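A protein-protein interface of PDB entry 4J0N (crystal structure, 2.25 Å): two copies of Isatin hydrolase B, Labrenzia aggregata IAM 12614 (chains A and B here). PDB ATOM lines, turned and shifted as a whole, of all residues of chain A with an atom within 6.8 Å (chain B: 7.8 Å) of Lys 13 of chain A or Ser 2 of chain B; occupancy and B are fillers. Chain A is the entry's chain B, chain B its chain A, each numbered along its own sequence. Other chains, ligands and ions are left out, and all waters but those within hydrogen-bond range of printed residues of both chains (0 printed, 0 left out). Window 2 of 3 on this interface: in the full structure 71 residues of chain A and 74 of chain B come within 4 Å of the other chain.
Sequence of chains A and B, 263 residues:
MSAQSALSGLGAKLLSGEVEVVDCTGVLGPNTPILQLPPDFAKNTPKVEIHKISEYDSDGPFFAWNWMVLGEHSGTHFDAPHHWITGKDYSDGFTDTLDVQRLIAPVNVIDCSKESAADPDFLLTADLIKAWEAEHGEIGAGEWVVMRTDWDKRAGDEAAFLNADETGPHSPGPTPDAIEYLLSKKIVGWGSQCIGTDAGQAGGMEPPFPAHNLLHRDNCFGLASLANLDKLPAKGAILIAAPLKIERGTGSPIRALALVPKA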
ATOM      1  N   SER A   8      -7.706  31.441 -34.448  1.00  0.00           N
ATOM      2  CA  SER A   8      -7.253  30.696 -35.616  1.00  0.00           C
ATOM      3  C   SER A   8      -5.843  30.162 -35.376  1.00  0.00           C
ATOM      4  O   SER A   8      -5.553  28.993 -35.659  1.00  0.00           O
ATOM      5  CB  SER A   8      -7.269  31.588 -36.858  1.00  0.00           C
ATOM      6  OG  SER A   8      -8.520  32.230 -37.009  1.00  0.00           O
ATOM      7  N   GLY A   9      -4.969  31.022 -34.857  1.00  0.00           N
ATOM      8  CA  GLY A   9      -3.632  30.600 -34.482  1.00  0.00           C
ATOM      9  C   GLY A   9      -3.682  29.390 -33.565  1.00  0.00           C
ATOM     10  O   GLY A   9      -2.993  28.390 -33.804  1.00  0.00           O
ATOM     11  N   LEU A  10      -4.526  29.471 -32.535  1.00  0.00           N
ATOM     12  CA  LEU A  10      -4.722  28.361 -31.594  1.00  0.00           C
ATOM     13  C   LEU A  10      -5.244  27.077 -32.257  1.00  0.00           C
ATOM     14  O   LEU A  10      -4.731  25.978 -32.002  1.00  0.00           O
ATOM     15  CB  LEU A  10      -5.661  28.781 -30.458  1.00  0.00           C
ATOM     16  CG  LEU A  10      -5.952  27.715 -29.396  1.00  0.00           C
ATOM     17  CD1 LEU A  10      -4.671  27.295 -28.676  1.00  0.00           C
ATOM     18  CD2 LEU A  10      -7.010  28.206 -28.403  1.00  0.00           C
ATOM     19  N   GLY A  11      -6.266  27.213 -33.096  1.00  0.00           N
ATOM     20  CA  GLY A  11      -6.783  26.066 -33.824  1.00  0.00           C
ATOM     21  C   GLY A  11      -5.706  25.359 -34.631  1.00  0.00           C
ATOM     22  O   GLY A  11      -5.635  24.127 -34.645  1.00  0.00           O
ATOM     23  N   ALA A  12      -4.855  26.133 -35.301  1.00  0.00           N
ATOM     24  CA  ALA A  12      -3.799  25.542 -36.124  1.00  0.00           C
ATOM     25  C   ALA A  12      -2.745  24.800 -35.284  1.00  0.00           C
ATOM     26  O   ALA A  12      -2.316  23.686 -35.643  1.00  0.00           O
ATOM     27  CB  ALA A  12      -3.148  26.611 -37.011  1.00  0.00           C
ATOM     28  N   LYS A  13      -2.334  25.417 -34.171  1.00  0.00           N
ATOM     29  CA  LYS A  13      -1.329  24.830 -33.277  1.00  0.00           C
ATOM     30  C   LYS A  13      -1.838  23.583 -32.551  1.00  0.00           C
ATOM     31  O   LYS A  13      -1.059  22.692 -32.212  1.00  0.00           O
ATOM     32  CB  LYS A  13      -0.819  25.883 -32.274  1.00  0.00           C
ATOM     33  CG  LYS A  13      -0.121  27.059 -32.946  1.00  0.00           C
ATOM     34  CD  LYS A  13       0.548  27.983 -31.937  1.00  0.00           C
ATOM     35  CE  LYS A  13       1.400  29.058 -32.628  1.00  0.00           C
ATOM     36  NZ  LYS A  13       0.646  29.904 -33.595  1.00  0.00           N
ATOM     37  N   LEU A  14      -3.146  23.537 -32.301  1.00  0.00           N
ATOM     38  CA  LEU A  14      -3.763  22.327 -31.775  1.00  0.00           C
ATOM     39  C   LEU A  14      -3.655  21.215 -32.810  1.00  0.00           C
ATOM     40  O   LEU A  14      -3.160  20.129 -32.504  1.00  0.00           O
ATOM     41  CB  LEU A  14      -5.224  22.574 -31.400  1.00  0.00           C
ATOM     42  CG  LEU A  14      -5.465  23.304 -30.078  1.00  0.00           C
ATOM     43  CD1 LEU A  14      -6.956  23.578 -29.868  1.00  0.00           C
ATOM     44  CD2 LEU A  14      -4.885  22.497 -28.909  1.00  0.00           C
ATOM     45  N   LEU A  15      -4.083  21.508 -34.039  1.00  0.00           N
ATOM     46  CA  LEU A  15      -4.086  20.529 -35.127  1.00  0.00           C
ATOM     47  C   LEU A  15      -2.686  20.002 -35.441  1.00  0.00           C
ATOM     48  O   LEU A  15      -2.527  18.831 -35.783  1.00  0.00           O
ATOM     49  CB  LEU A  15      -4.744  21.127 -36.382  1.00  0.00           C
ATOM     50  CG  LEU A  15      -6.284  21.107 -36.514  1.00  0.00           C
ATOM     51  CD1 LEU A  15      -7.023  21.394 -35.209  1.00  0.00           C
ATOM     52  CD2 LEU A  15      -6.783  22.079 -37.591  1.00  0.00           C
ATOM     53  N   SER A  16      -1.681  20.866 -35.295  1.00  0.00           N
ATOM     54  CA  SER A  16      -0.277  20.513 -35.562  1.00  0.00           C
ATOM     55  C   SER A  16       0.450  19.925 -34.344  1.00  0.00           C
ATOM     56  O   SER A  16       1.526  19.336 -34.479  1.00  0.00           O
ATOM     57  CB  SER A  16       0.495  21.748 -36.023  1.00  0.00           C
ATOM     58  OG  SER A  16       0.857  22.575 -34.919  1.00  0.00           O
ATOM     59  N   GLY A  17      -0.120  20.110 -33.154  1.00  0.00           N
ATOM     60  CA  GLY A  17       0.498  19.595 -31.945  1.00  0.00           C
ATOM     61  C   GLY A  17       1.567  20.506 -31.364  1.00  0.00           C
ATOM     62  O   GLY A  17       2.328  20.091 -30.488  1.00  0.00           O
ATOM     63  N   GLU A  18       1.640  21.741 -31.859  1.00  0.00           N
ATOM     64  CA  GLU A  18       2.516  22.751 -31.263  1.00  0.00           C
ATOM     65  C   GLU A  18       1.950  23.225 -29.923  1.00  0.00           C
ATOM     66  O   GLU A  18       2.686  23.707 -29.065  1.00  0.00           O
ATOM     67  CB  GLU A  18       2.667  23.953 -32.192  1.00  0.00           C
ATOM     68  CG  GLU A  18       3.537  23.733 -33.418  1.00  0.00           C
ATOM     69  CD  GLU A  18       3.437  24.910 -34.390  1.00  0.00           C
ATOM     70  OE1 GLU A  18       2.563  24.857 -35.296  1.00  0.00           O
ATOM     71  OE2 GLU A  18       4.213  25.888 -34.232  1.00  0.00           O
ATOM     72  N   VAL A  19       0.630  23.126 -29.775  1.00  0.00           N
ATOM     73  CA  VAL A  19      -0.009  23.232 -28.466  1.00  0.00           C
ATOM     74  C   VAL A  19      -0.553  21.858 -28.110  1.00  0.00           C
ATOM     75  O   VAL A  19      -1.404  21.313 -28.833  1.00  0.00           O
ATOM     76  CB  VAL A  19      -1.160  24.248 -28.446  1.00  0.00           C
ATOM     77  CG1 VAL A  19      -1.984  24.088 -27.161  1.00  0.00           C
ATOM     78  CG2 VAL A  19      -0.618  25.662 -28.552  1.00  0.00           C
ATOM     79  N   GLU A  20      -0.041  21.296 -27.017  1.00  0.00           N
ATOM     80  CA  GLU A  20      -0.440  19.958 -26.566  1.00  0.00           C
ATOM     81  C   GLU A  20      -1.591  20.003 -25.559  1.00  0.00           C
ATOM     82  O   GLU A  20      -1.604  20.835 -24.639  1.00  0.00           O
ATOM     83  CB  GLU A  20       0.750  19.229 -25.932  1.00  0.00           C
ATOM     84  CG  GLU A  20       1.409  18.191 -26.832  1.00  0.00           C
ATOM     85  CD  GLU A  20       2.805  17.774 -26.353  1.00  0.00           C
ATOM     86  OE1 GLU A  20       3.033  17.699 -25.117  1.00  0.00           O
ATOM     87  OE2 GLU A  20       3.674  17.524 -27.226  1.00  0.00           O
ATOM     88  N   PRO A 261       2.588  24.320 -24.220  1.00  0.00           N
ATOM     89  CA  PRO A 261       3.437  24.329 -25.418  1.00  0.00           C
ATOM     90  C   PRO A 261       4.156  22.997 -25.588  1.00  0.00           C
ATOM     91  O   PRO A 261       4.574  22.437 -24.572  1.00  0.00           O
ATOM     92  CB  PRO A 261       4.470  25.421 -25.111  1.00  0.00           C
ATOM     93  CG  PRO A 261       4.484  25.531 -23.617  1.00  0.00           C
ATOM     94  CD  PRO A 261       3.076  25.245 -23.178  1.00  0.00           C
ATOM     95  N   SER B   2       5.114  31.460 -31.800  1.00  0.00           N
ATOM     96  CA  SER B   2       5.462  30.702 -30.595  1.00  0.00           C
ATOM     97  C   SER B   2       4.190  30.177 -29.921  1.00  0.00           C
ATOM     98  O   SER B   2       3.202  30.904 -29.782  1.00  0.00           O
ATOM     99  CB  SER B   2       6.272  31.578 -29.626  1.00  0.00           C
ATOM    100  OG  SER B   2       6.551  30.929 -28.396  1.00  0.00           O
ATOM    101  N   ALA B   3       4.207  28.908 -29.529  1.00  0.00           N
ATOM    102  CA  ALA B   3       3.079  28.322 -28.807  1.00  0.00           C
ATOM    103  C   ALA B   3       2.833  29.057 -27.486  1.00  0.00           C
ATOM    104  O   ALA B   3       1.690  29.320 -27.108  1.00  0.00           O
ATOM    105  CB  ALA B   3       3.327  26.836 -28.554  1.00  0.00           C
ATOM    106  N   GLN B   4       3.912  29.388 -26.792  1.00  0.00           N
ATOM    107  CA  GLN B   4       3.795  30.040 -25.512  1.00  0.00           C
ATOM    108  C   GLN B   4       3.221  31.441 -25.667  1.00  0.00           C
ATOM    109  O   GLN B   4       2.334  31.842 -24.904  1.00  0.00           O
ATOM    110  CB  GLN B   4       5.146  30.083 -24.798  1.00  0.00           C
ATOM    111  CG  GLN B   4       5.033  30.514 -23.338  1.00  0.00           C
ATOM    112  CD  GLN B   4       3.920  29.775 -22.613  1.00  0.00           C
ATOM    113  OE1 GLN B   4       4.041  28.581 -22.318  1.00  0.00           O
ATOM    114  NE2 GLN B   4       2.817  30.475 -22.343  1.00  0.00           N
ATOM    115  N   SER B   5       3.707  32.184 -26.658  1.00  0.00           N
ATOM    116  CA  SER B   5       3.193  33.534 -26.885  1.00  0.00           C
ATOM    117  C   SER B   5       1.715  33.489 -27.262  1.00  0.00           C
ATOM    118  O   SER B   5       0.951  34.412 -26.962  1.00  0.00           O
ATOM    119  CB  SER B   5       4.017  34.274 -27.945  1.00  0.00           C
ATOM    120  OG  SER B   5       4.015  33.576 -29.174  1.00  0.00           O
ATOM    121  N   ALA B   6       1.312  32.396 -27.899  1.00  0.00           N
ATOM    122  CA  ALA B   6      -0.089  32.180 -28.241  1.00  0.00           C
ATOM    123  C   ALA B   6      -0.943  31.897 -26.994  1.00  0.00           C
ATOM    124  O   ALA B   6      -2.031  32.463 -26.833  1.00  0.00           O
ATOM    125  CB  ALA B   6      -0.208  31.044 -29.245  1.00  0.00           C
ATOM    126  N   LEU B   7      -0.455  31.014 -26.120  1.00  0.00           N
ATOM    127  CA  LEU B   7      -1.178  30.683 -24.883  1.00  0.00           C
ATOM    128  C   LEU B   7      -1.331  31.901 -23.946  1.00  0.00           C
ATOM    129  O   LEU B   7      -2.408  32.139 -23.382  1.00  0.00           O
ATOM    130  CB  LEU B   7      -0.521  29.500 -24.153  1.00  0.00           C
ATOM    131  CG  LEU B   7      -0.524  28.131 -24.852  1.00  0.00           C
ATOM    132  CD1 LEU B   7       0.350  27.157 -24.099  1.00  0.00           C
ATOM    133  CD2 LEU B   7      -1.936  27.552 -25.024  1.00  0.00           C
ATOM    134  N   SER B   8      -0.265  32.681 -23.800  1.00  0.00           N
ATOM    135  CA  SER B   8      -0.323  33.879 -22.962  1.00  0.00           C
ATOM    136  C   SER B   8      -1.323  34.884 -23.528  1.00  0.00           C
ATOM    137  O   SER B   8      -2.133  35.453 -22.793  1.00  0.00           O
ATOM    138  CB  SER B   8       1.056  34.523 -22.876  1.00  0.00           C
ATOM    139  OG  SER B   8       2.033  33.547 -22.587  1.00  0.00           O
ATOM    140  N   GLN B 101      -6.193  15.190 -27.476  1.00  0.00           N
ATOM    141  CA  GLN B 101      -5.685  16.159 -28.451  1.00  0.00           C
ATOM    142  C   GLN B 101      -6.775  16.523 -29.476  1.00  0.00           C
ATOM    143  O   GLN B 101      -6.864  17.667 -29.932  1.00  0.00           O
ATOM    144  CB  GLN B 101      -4.443  15.606 -29.163  1.00  0.00           C
ATOM    145  CG  GLN B 101      -3.701  16.627 -30.036  1.00  0.00           C
ATOM    146  CD  GLN B 101      -3.082  17.766 -29.205  1.00  0.00           C
ATOM    147  OE1 GLN B 101      -2.889  17.628 -27.989  1.00  0.00           O
ATOM    148  NE2 GLN B 101      -2.769  18.886 -29.859  1.00  0.00           N
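Position printed for both chains: 8.
Of the 9 pairs that touch across the chains among the printed residues, none has its exchanged pair printed and touching as well.
Printed residues of chain A that touch a printed residue of chain B: Lys 13, Leu 14, Gly 17, Glu 18, Val 19, Glu 20 and Pro 261.
Hydrophobic or aromatic side chains of chain A within 4 Å of the printed part of chain B: Pro 261.
Of the 8 printed residues of chain B, 5 touch a printed residue of chain A.
Hydrophobic or aromatic side chains of chain B that line the printed part of chain A: Ala 3 and Leu 7.
Among the printed residues, no Asp or Glu carboxylate lies within 4 Å of a Lys or Arg side-chain nitrogen of the other chain.
Among the printed residues, merely in contact across the chains: Glu 18 of chain A with Ala 3 of chain B (3.2 Å), Pro 261 of chain A with Gln 4 of chain B (3.3 Å), Pro 261 of chain A with Leu 7 of chain B (3.5 Å), Glu 20 of chain A with Gln 101 of chain B (3.6 Å), Lys 13 of chain A with Ser 2 of chain B (3.8 Å), Pro 261 of chain A with Ala 3 of chain B (3.9 Å) and Gly 17 of chain A with Gln 101 of chain B (3.9 Å).
O of Leu 14 of chain A sits at hydrogen-bond distance from NE2 of Gln 101 of chain B (2.9 Å).
The side-chain amide nitrogen (NE2) of Gln 101 of chain B lies within hydrogen-bond range of the backbone carbonyl oxygen (O) of Val 19 of chain A (3.0 Å).
O of Ser 2 of chain B is in hydrogen-bond range of OG of Ser 5 of chain B, at 2.9 Å.
OG of Ser 16 of chain A is in hydrogen-bond range of OE1 of Glu 18 of chain A (2.9 Å).
The backbone carbonyl oxygen (O) of Lys 13 of chain A sits at hydrogen-bond distance from the backbone NH (N) of Glu 18 of chain A (2.9 Å).
O of Lys 13 of chain A lies within hydrogen-bond range of N of Val 19 of chain A, at 3.0 Å.
The backbone carbonyl oxygen of Lys 13 of chain A is in hydrogen-bond range of the side-chain hydroxyl of Ser 16 of chain A, at 3.3 Å.
The backbone NH (N) of Gln 4 of chain B sits close to the side-chain hydroxyl (OG) of Ser 2 of chain B.
Lys 13 of chain A touches just one residue of chain B: Ser 2.
Ser 2 of chain B touches one residue of chain A.
Printed residues of chain A within 4 Å of Gln 101 of chain B: Leu 14, Gly 17, Val 19 and Glu 20.
Of the printed residues of chain B, Val 19 of chain A touches Gln 101 (3.0 Å).
Printed residues of chain A within 4 Å of Ala 3 of chain B: Glu 18 (3.2 Å) and Pro 261 (3.9 Å).
Ser 8 of chain B touches none of the printed residues of chain A.
Ala 6 of chain B touches none of the printed residues of chain A.
The nearest residue of chain B that does not touch Lys 13 of chain A is Ala 3 of chain B (4.04 Å).
The nearest residue of chain A that does not touch Ser 2 of chain B is Glu 18 of chain A (6.1 Å).
The nearest printed residue of chain B that does not touch Val 19 of chain A is Leu 7 of chain B (4.1 Å).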
